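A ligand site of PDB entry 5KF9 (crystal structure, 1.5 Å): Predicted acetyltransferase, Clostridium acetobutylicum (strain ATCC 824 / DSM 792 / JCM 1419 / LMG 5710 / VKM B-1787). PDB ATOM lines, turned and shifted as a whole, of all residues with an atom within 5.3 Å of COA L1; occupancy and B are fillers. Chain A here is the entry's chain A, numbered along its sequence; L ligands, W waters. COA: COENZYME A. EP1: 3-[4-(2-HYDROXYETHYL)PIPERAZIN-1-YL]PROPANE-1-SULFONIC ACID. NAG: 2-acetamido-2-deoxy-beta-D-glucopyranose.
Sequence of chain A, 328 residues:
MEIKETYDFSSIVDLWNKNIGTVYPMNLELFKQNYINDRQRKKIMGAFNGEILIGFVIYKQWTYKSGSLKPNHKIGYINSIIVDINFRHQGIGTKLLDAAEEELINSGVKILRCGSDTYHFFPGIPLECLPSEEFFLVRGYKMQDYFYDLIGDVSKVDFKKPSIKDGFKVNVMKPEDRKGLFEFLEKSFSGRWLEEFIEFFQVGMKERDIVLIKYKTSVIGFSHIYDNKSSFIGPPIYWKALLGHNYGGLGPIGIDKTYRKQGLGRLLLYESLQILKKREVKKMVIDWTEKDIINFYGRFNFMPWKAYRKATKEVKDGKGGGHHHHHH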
ATOM      1  N   PHE A 189       6.289 -16.497   3.058  1.00  0.00           N
ATOM      2  CA  PHE A 189       7.306 -16.156   4.033  1.00  0.00           C
ATOM      3  C   PHE A 189       8.102 -17.408   4.327  1.00  0.00           C
ATOM      4  O   PHE A 189       8.166 -17.859   5.473  1.00  0.00           O
ATOM      5  CB  PHE A 189       6.707 -15.586   5.326  1.00  0.00           C
ATOM      6  CG  PHE A 189       5.997 -14.316   5.141  1.00  0.00           C
ATOM      7  CD1 PHE A 189       6.668 -13.154   4.849  1.00  0.00           C
ATOM      8  CD2 PHE A 189       4.615 -14.294   5.251  1.00  0.00           C
ATOM      9  CE1 PHE A 189       5.997 -11.991   4.620  1.00  0.00           C
ATOM     10  CE2 PHE A 189       3.922 -13.131   4.999  1.00  0.00           C
ATOM     11  CZ  PHE A 189       4.619 -11.954   4.761  1.00  0.00           C
ATOM     12  N   TRP A 193      11.129 -16.786   8.714  1.00  0.00           N
ATOM     13  CA  TRP A 193       9.905 -16.859   9.479  1.00  0.00           C
ATOM     14  C   TRP A 193       9.314 -18.240   9.447  1.00  0.00           C
ATOM     15  O   TRP A 193       8.751 -18.653  10.450  1.00  0.00           O
ATOM     16  CB  TRP A 193       8.937 -15.810   9.001  1.00  0.00           C
ATOM     17  CG  TRP A 193       9.317 -14.396   9.412  1.00  0.00           C
ATOM     18  CD1 TRP A 193      10.356 -14.012  10.190  1.00  0.00           C
ATOM     19  CD2 TRP A 193       8.573 -13.227   9.126  1.00  0.00           C
ATOM     20  NE1 TRP A 193      10.351 -12.633  10.326  1.00  0.00           N
ATOM     21  CE2 TRP A 193       9.257 -12.131   9.687  1.00  0.00           C
ATOM     22  CE3 TRP A 193       7.429 -12.975   8.368  1.00  0.00           C
ATOM     23  CZ2 TRP A 193       8.826 -10.815   9.528  1.00  0.00           C
ATOM     24  CZ3 TRP A 193       6.993 -11.668   8.239  1.00  0.00           C
ATOM     25  CH2 TRP A 193       7.659 -10.618   8.845  1.00  0.00           C
ATOM     26  N   ILE A 253       4.857 -10.077  11.928  1.00  0.00           N
ATOM     27  CA  ILE A 253       3.543  -9.778  11.363  1.00  0.00           C
ATOM     28  C   ILE A 253       3.680  -9.684   9.852  1.00  0.00           C
ATOM     29  O   ILE A 253       4.576  -9.024   9.332  1.00  0.00           O
ATOM     30  CB  ILE A 253       2.864  -8.548  11.991  1.00  0.00           C
ATOM     31  CG1 ILE A 253       1.483  -8.319  11.378  1.00  0.00           C
ATOM     32  CG2 ILE A 253       3.804  -7.346  11.871  1.00  0.00           C
ATOM     33  CD1 ILE A 253       0.685  -7.344  12.181  1.00  0.00           C
ATOM     34  N   GLY A 254       2.867 -10.425   9.125  1.00  0.00           N
ATOM     35  CA  GLY A 254       2.998 -10.465   7.679  1.00  0.00           C
ATOM     36  C   GLY A 254       1.668 -10.740   7.009  1.00  0.00           C
ATOM     37  O   GLY A 254       0.866 -11.502   7.526  1.00  0.00           O
ATOM     38  N   ILE A 255       1.499 -10.139   5.830  1.00  0.00           N
ATOM     39  CA  ILE A 255       0.380 -10.287   4.912  1.00  0.00           C
ATOM     40  C   ILE A 255       0.923 -10.771   3.553  1.00  0.00           C
ATOM     41  O   ILE A 255       1.947 -10.316   3.102  1.00  0.00           O
ATOM     42  CB  ILE A 255      -0.357  -8.925   4.713  1.00  0.00           C
ATOM     43  CG1 ILE A 255      -0.981  -8.460   6.013  1.00  0.00           C
ATOM     44  CG2 ILE A 255      -1.258  -8.909   3.482  1.00  0.00           C
ATOM     45  CD1 ILE A 255      -2.177  -9.240   6.481  1.00  0.00           C
ATOM     46  N   TYR A 259      -2.051  -9.195  -1.295  1.00  0.00           N
ATOM     47  CA  TYR A 259      -3.101  -8.579  -0.468  1.00  0.00           C
ATOM     48  C   TYR A 259      -2.661  -7.296   0.242  1.00  0.00           C
ATOM     49  O   TYR A 259      -3.366  -6.746   1.062  1.00  0.00           O
ATOM     50  CB  TYR A 259      -3.628  -9.580   0.592  1.00  0.00           C
ATOM     51  CG  TYR A 259      -4.546 -10.644   0.032  1.00  0.00           C
ATOM     52  CD1 TYR A 259      -5.912 -10.426  -0.083  1.00  0.00           C
ATOM     53  CD2 TYR A 259      -4.055 -11.870  -0.382  1.00  0.00           C
ATOM     54  CE1 TYR A 259      -6.758 -11.387  -0.592  1.00  0.00           C
ATOM     55  CE2 TYR A 259      -4.882 -12.840  -0.920  1.00  0.00           C
ATOM     56  CZ  TYR A 259      -6.234 -12.593  -1.005  1.00  0.00           C
ATOM     57  OH  TYR A 259      -7.055 -13.575  -1.533  1.00  0.00           O
ATOM     58  N   ARG A 260      -1.450  -6.847  -0.024  1.00  0.00           N
ATOM     59  CA  ARG A 260      -0.913  -5.704   0.669  1.00  0.00           C
ATOM     60  C   ARG A 260      -1.489  -4.379   0.183  1.00  0.00           C
ATOM     61  O   ARG A 260      -2.093  -4.323  -0.886  1.00  0.00           O
ATOM     62  CB  ARG A 260       0.610  -5.696   0.547  1.00  0.00           C
ATOM     63  CG  ARG A 260       1.232  -6.668   1.553  1.00  0.00           C
ATOM     64  CD  ARG A 260       2.749  -6.737   1.481  1.00  0.00           C
ATOM     65  NE  ARG A 260       3.224  -8.074   1.818  1.00  0.00           N
ATOM     66  CZ  ARG A 260       4.422  -8.592   1.537  1.00  0.00           C
ATOM     67  NH1 ARG A 260       5.353  -7.866   0.917  1.00  0.00           N
ATOM     68  NH2 ARG A 260       4.702  -9.859   1.898  1.00  0.00           N
ATOM     69  N   LYS A 261      -1.278  -3.335   0.972  1.00  0.00           N
ATOM     70  CA  LYS A 261      -1.735  -1.984   0.684  1.00  0.00           C
ATOM     71  C   LYS A 261      -3.245  -1.872   0.458  1.00  0.00           C
ATOM     72  O   LYS A 261      -3.715  -0.972  -0.264  1.00  0.00           O
ATOM     73  CB  LYS A 261      -0.950  -1.396  -0.495  1.00  0.00           C
ATOM     74  CG  LYS A 261       0.533  -1.255  -0.200  1.00  0.00           C
ATOM     75  CD  LYS A 261       0.770  -0.355   0.996  1.00  0.00           C
ATOM     76  CE  LYS A 261       2.198   0.158   1.050  1.00  0.00           C
ATOM     77  NZ  LYS A 261       2.256   1.351   1.937  1.00  0.00           N
ATOM     78  N   GLN A 262      -4.007  -2.744   1.120  1.00  0.00           N
ATOM     79  CA  GLN A 262      -5.467  -2.693   1.154  1.00  0.00           C
ATOM     80  C   GLN A 262      -6.043  -2.471   2.552  1.00  0.00           C
ATOM     81  O   GLN A 262      -7.250  -2.539   2.740  1.00  0.00           O
ATOM     82  CB  GLN A 262      -6.036  -4.022   0.669  1.00  0.00           C
ATOM     83  CG  GLN A 262      -5.668  -4.422  -0.745  1.00  0.00           C
ATOM     84  CD  GLN A 262      -6.340  -5.728  -1.132  1.00  0.00           C
ATOM     85  OE1 GLN A 262      -7.407  -6.057  -0.631  1.00  0.00           O
ATOM     86  NE2 GLN A 262      -5.716  -6.471  -2.029  1.00  0.00           N
ATOM     87  N   GLY A 263      -5.224  -2.272   3.588  1.00  0.00           N
ATOM     88  CA  GLY A 263      -5.756  -2.068   4.930  1.00  0.00           C
ATOM     89  C   GLY A 263      -5.761  -3.300   5.846  1.00  0.00           C
ATOM     90  O   GLY A 263      -6.196  -3.204   6.996  1.00  0.00           O
ATOM     91  N   LEU A 264      -5.372  -4.414   5.258  1.00  0.00           N
ATOM     92  CA  LEU A 264      -5.463  -5.711   5.906  1.00  0.00           C
ATOM     93  C   LEU A 264      -4.365  -5.837   6.970  1.00  0.00           C
ATOM     94  O   LEU A 264      -4.582  -6.451   7.999  1.00  0.00           O
ATOM     95  CB  LEU A 264      -5.489  -6.863   4.932  1.00  0.00           C
ATOM     96  CG  LEU A 264      -6.675  -6.787   3.935  1.00  0.00           C
ATOM     97  CD1 LEU A 264      -6.450  -7.663   2.707  1.00  0.00           C
ATOM     98  CD2 LEU A 264      -7.967  -7.117   4.677  1.00  0.00           C
ATOM     99  N   GLY A 265      -3.182  -5.268   6.747  1.00  0.00           N
ATOM    100  CA  GLY A 265      -2.167  -5.317   7.798  1.00  0.00           C
ATOM    101  C   GLY A 265      -2.624  -4.503   8.982  1.00  0.00           C
ATOM    102  O   GLY A 265      -2.486  -4.885  10.144  1.00  0.00           O
ATOM    103  N   ARG A 266      -3.239  -3.324   8.751  1.00  0.00           N
ATOM    104  CA  ARG A 266      -3.774  -2.527   9.831  1.00  0.00           C
ATOM    105  C   ARG A 266      -4.859  -3.284  10.634  1.00  0.00           C
ATOM    106  O   ARG A 266      -4.920  -3.255  11.851  1.00  0.00           O
ATOM    107  CB  ARG A 266      -4.270  -1.180   9.299  1.00  0.00           C
ATOM    108  CG  ARG A 266      -4.827  -0.253  10.345  1.00  0.00           C
ATOM    109  CD  ARG A 266      -4.986   1.145   9.752  1.00  0.00           C
ATOM    110  NE  ARG A 266      -6.311   1.688   9.967  1.00  0.00           N
ATOM    111  CZ  ARG A 266      -6.737   2.857   9.497  1.00  0.00           C
ATOM    112  NH1 ARG A 266      -5.917   3.637   8.795  1.00  0.00           N
ATOM    113  NH2 ARG A 266      -7.977   3.257   9.737  1.00  0.00           N
ATOM    114  N   LEU A 267      -5.721  -3.967   9.879  1.00  0.00           N
ATOM    115  CA  LEU A 267      -6.785  -4.756  10.527  1.00  0.00           C
ATOM    116  C   LEU A 267      -6.151  -5.861  11.396  1.00  0.00           C
ATOM    117  O   LEU A 267      -6.552  -6.045  12.553  1.00  0.00           O
ATOM    118  CB  LEU A 267      -7.703  -5.384   9.483  1.00  0.00           C
ATOM    119  CG  LEU A 267      -8.813  -6.265  10.109  1.00  0.00           C
ATOM    120  CD1 LEU A 267      -9.690  -5.400  11.021  1.00  0.00           C
ATOM    121  CD2 LEU A 267      -9.564  -6.991   8.994  1.00  0.00           C
ATOM    122  N   ILE A 293       8.835   1.502   8.292  1.00  0.00           N
ATOM    123  CA  ILE A 293       7.585   0.924   8.786  1.00  0.00           C
ATOM    124  C   ILE A 293       7.181   1.420  10.160  1.00  0.00           C
ATOM    125  O   ILE A 293       6.085   1.113  10.666  1.00  0.00           O
ATOM    126  CB  ILE A 293       7.573  -0.642   8.748  1.00  0.00           C
ATOM    127  CG1 ILE A 293       6.115  -1.195   8.735  1.00  0.00           C
ATOM    128  CG2 ILE A 293       8.385  -1.204   9.896  1.00  0.00           C
ATOM    129  CD1 ILE A 293       5.302  -0.816   7.507  1.00  0.00           C
ATOM    130  N   PHE A 296       3.587   2.861  10.677  1.00  0.00           N
ATOM    131  CA  PHE A 296       2.514   1.843  10.681  1.00  0.00           C
ATOM    132  C   PHE A 296       2.160   1.455  12.115  1.00  0.00           C
ATOM    133  O   PHE A 296       0.988   1.429  12.523  1.00  0.00           O
ATOM    134  CB  PHE A 296       2.963   0.625   9.884  1.00  0.00           C
ATOM    135  CG  PHE A 296       2.047  -0.571   9.959  1.00  0.00           C
ATOM    136  CD1 PHE A 296       0.837  -0.572   9.298  1.00  0.00           C
ATOM    137  CD2 PHE A 296       2.479  -1.722  10.581  1.00  0.00           C
ATOM    138  CE1 PHE A 296       0.029  -1.683   9.365  1.00  0.00           C
ATOM    139  CE2 PHE A 296       1.693  -2.869  10.597  1.00  0.00           C
ATOM    140  CZ  PHE A 296       0.455  -2.828   9.997  1.00  0.00           C
ATOM    141  N   TYR A 297       3.154   1.218  12.957  1.00  0.00           N
ATOM    142  CA  TYR A 297       2.939   0.931  14.344  1.00  0.00           C
ATOM    143  C   TYR A 297       2.707   2.199  15.173  1.00  0.00           C
ATOM    144  O   TYR A 297       2.046   2.191  16.196  1.00  0.00           O
ATOM    145  CB  TYR A 297       4.134   0.138  14.889  1.00  0.00           C
ATOM    146  CG  TYR A 297       4.447  -1.104  14.134  1.00  0.00           C
ATOM    147  CD1 TYR A 297       3.657  -2.242  14.281  1.00  0.00           C
ATOM    148  CD2 TYR A 297       5.492  -1.172  13.227  1.00  0.00           C
ATOM    149  CE1 TYR A 297       3.886  -3.374  13.549  1.00  0.00           C
ATOM    150  CE2 TYR A 297       5.746  -2.335  12.518  1.00  0.00           C
ATOM    151  CZ  TYR A 297       4.963  -3.421  12.724  1.00  0.00           C
ATOM    152  OH  TYR A 297       5.212  -4.555  11.977  1.00  0.00           O
HETATM  153  O5B COA L   1      -2.795  -2.030   6.347  1.00  0.00           O
HETATM  154  P1A COA L   1      -1.766  -1.660   5.195  1.00  0.00           P
HETATM  155  O1A COA L   1      -1.280  -0.310   5.635  1.00  0.00           O
HETATM  156  O2A COA L   1      -2.332  -1.718   3.808  1.00  0.00           O
HETATM  157  O3A COA L   1      -0.372  -2.498   5.092  1.00  0.00           O
HETATM  158  P2A COA L   1      -0.179  -3.891   4.385  1.00  0.00           P
HETATM  159  O4A COA L   1       0.762  -3.724   3.232  1.00  0.00           O
HETATM  160  O5A COA L   1      -1.434  -4.757   4.309  1.00  0.00           O
HETATM  161  O6A COA L   1       0.536  -4.554   5.671  1.00  0.00           O
HETATM  162  CBP COA L   1       2.641  -5.216   6.494  1.00  0.00           C
HETATM  163  CCP COA L   1       1.742  -4.043   6.238  1.00  0.00           C
HETATM  164  CDP COA L   1       1.820  -6.297   7.166  1.00  0.00           C
HETATM  165  CEP COA L   1       3.728  -4.961   7.507  1.00  0.00           C
HETATM  166  CAP COA L   1       3.016  -5.819   5.136  1.00  0.00           C
HETATM  167  OAP COA L   1       3.635  -4.886   4.239  1.00  0.00           O
HETATM  168  C9P COA L   1       3.876  -7.043   5.119  1.00  0.00           C
HETATM  169  O9P COA L   1       3.496  -8.194   5.336  1.00  0.00           O
HETATM  170  N8P COA L   1       5.139  -6.866   4.718  1.00  0.00           N
HETATM  171  C7P COA L   1       6.006  -8.007   4.499  1.00  0.00           C
HETATM  172  C6P COA L   1       6.788  -8.308   5.765  1.00  0.00           C
HETATM  173  C5P COA L   1       7.941  -7.324   5.811  1.00  0.00           C
HETATM  174  O5P COA L   1       8.790  -7.242   4.909  1.00  0.00           O
HETATM  175  N4P COA L   1       7.966  -6.573   6.905  1.00  0.00           N
HETATM  176  O2S EP1 L   2      10.682 -15.429   6.349  1.00  0.00           O
HETATM  177  S   EP1 L   2      11.155 -14.566   5.317  1.00  0.00           S
HETATM  178  O3S EP1 L   2      12.594 -14.553   5.389  1.00  0.00           O
HETATM  179  O1S EP1 L   2      10.748 -15.238   3.874  1.00  0.00           O
HETATM  180  C11 EP1 L   2      10.544 -13.029   5.411  1.00  0.00           C
HETATM  181  C10 EP1 L   2      11.574 -12.132   6.081  1.00  0.00           C
HETATM  182  C9  EP1 L   2      11.025 -10.728   6.262  1.00  0.00           C
HETATM  183  N1  EP1 L   2      11.730  -9.932   7.298  1.00  0.00           N
HETATM  184  C2  EP1 L   2      12.865 -10.542   8.035  1.00  0.00           C
HETATM  185  C3  EP1 L   2      13.509  -9.640   9.093  1.00  0.00           C
HETATM  186  N4  EP1 L   2      13.492  -8.204   8.714  1.00  0.00           N
HETATM  187  C5  EP1 L   2      12.392  -7.680   7.892  1.00  0.00           C
HETATM  188  C6  EP1 L   2      12.052  -8.619   6.748  1.00  0.00           C
HETATM  189  C7  EP1 L   2      14.062  -7.313   9.743  1.00  0.00           C
HETATM  190  C8  EP1 L   2      13.620  -5.863   9.676  1.00  0.00           C
HETATM  191  O8  EP1 L   2      12.276  -5.768  10.138  1.00  0.00           O
HETATM  192  C1  NAG L   3      11.453  -8.981  11.979  1.00  0.00           C
HETATM  193  C2  NAG L   3      10.233  -8.999  12.873  1.00  0.00           C
HETATM  194  C3  NAG L   3      10.632  -9.590  14.217  1.00  0.00           C
HETATM  195  C4  NAG L   3      11.382 -10.929  14.113  1.00  0.00           C
HETATM  196  C5  NAG L   3      12.524 -10.729  13.131  1.00  0.00           C
HETATM  197  C6  NAG L   3      13.372 -11.948  12.862  1.00  0.00           C
HETATM  198  C7  NAG L   3       8.340  -7.476  12.630  1.00  0.00           C
HETATM  199  C8  NAG L   3       7.649  -6.284  13.226  1.00  0.00           C
HETATM  200  N2  NAG L   3       9.592  -7.728  13.065  1.00  0.00           N
HETATM  201  O1  NAG L   3      11.092  -8.529  10.685  1.00  0.00           O
HETATM  202  O3  NAG L   3       9.434  -9.763  14.981  1.00  0.00           O
HETATM  203  O4  NAG L   3      11.856 -11.298  15.413  1.00  0.00           O
HETATM  204  O5  NAG L   3      11.965 -10.294  11.908  1.00  0.00           O
HETATM  205  O6  NAG L   3      12.544 -12.981  12.276  1.00  0.00           O
HETATM  206  O7  NAG L   3       7.691  -8.153  11.819  1.00  0.00           O
HETATM  207  O   HOH W   1      -3.478   0.872   2.781  1.00  0.00           O
HETATM  208  O   HOH W   2       6.612  -7.230   9.413  1.00  0.00           O
HETATM  209  O   HOH W   3      -3.479  -4.837   2.885  1.00  0.00           O
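An oxygen (O5B) of COA L1 sits at hydrogen-bond distance from the backbone NH (N) of Arg 266. N of Ile 255 is in hydrogen-bond range of O9P of COA L1 (2.8 Å). An oxygen (O2A) of COA L1 lies within hydrogen-bond range of the backbone NH (N) of Gly 263. An oxygen (O5A) of COA L1 sits at hydrogen-bond distance from the backbone NH (N) of Gly 265 (3.0 Å). The backbone NH (N) of Lys 261 sits at hydrogen-bond distance from an oxygen (O4A) of COA L1. The backbone NH of Gln 262 is in hydrogen-bond range of an oxygen (O2A) of COA L1 (3.3 Å). The backbone NH (N) of Trp 193 lies within hydrogen-bond range of an oxygen (O2S) of EP1 L2 (2.8 Å). The indole nitrogen of Trp 193 lies within hydrogen-bond range of an oxygen (O6) of NAG L3 (3.0 Å). The backbone NH (N) of Ile 253 is in hydrogen-bond range of an oxygen (O7) of NAG L3 (3.4 Å).
An oxygen (O8) of EP1 L2 sits at hydrogen-bond distance from an oxygen (O1) of NAG L3 (3.1 Å).
O of Ile 255 sits at hydrogen-bond distance from NE of Arg 260, at 2.9 Å.
Phe 189 touches COA L1. CH2 of Trp 193 touches C6P of COA L1, 3.9 Å away. CA of Gly 254 touches O9P of COA L1 (3.3 Å). Arg 260 touches COA L1. Leu 264 touches COA L1. Hydrophobic or aromatic side chains that line COA L1: Phe 189, Trp 193 and Ile 255. Within 4 Å of COA L1: Phe 189, Trp 193, Gly 254, Ile 255, Arg 260, Lys 261, Gln 262, Gly 263, Leu 264, Gly 265 and Arg 266. The nearest printed residue that does not touch COA L1 is Phe 296 (4.1 Å).
Water W2 lies within hydrogen-bond range of O of Ile 253, O7 of NAG L3 and N4P of COA L1.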
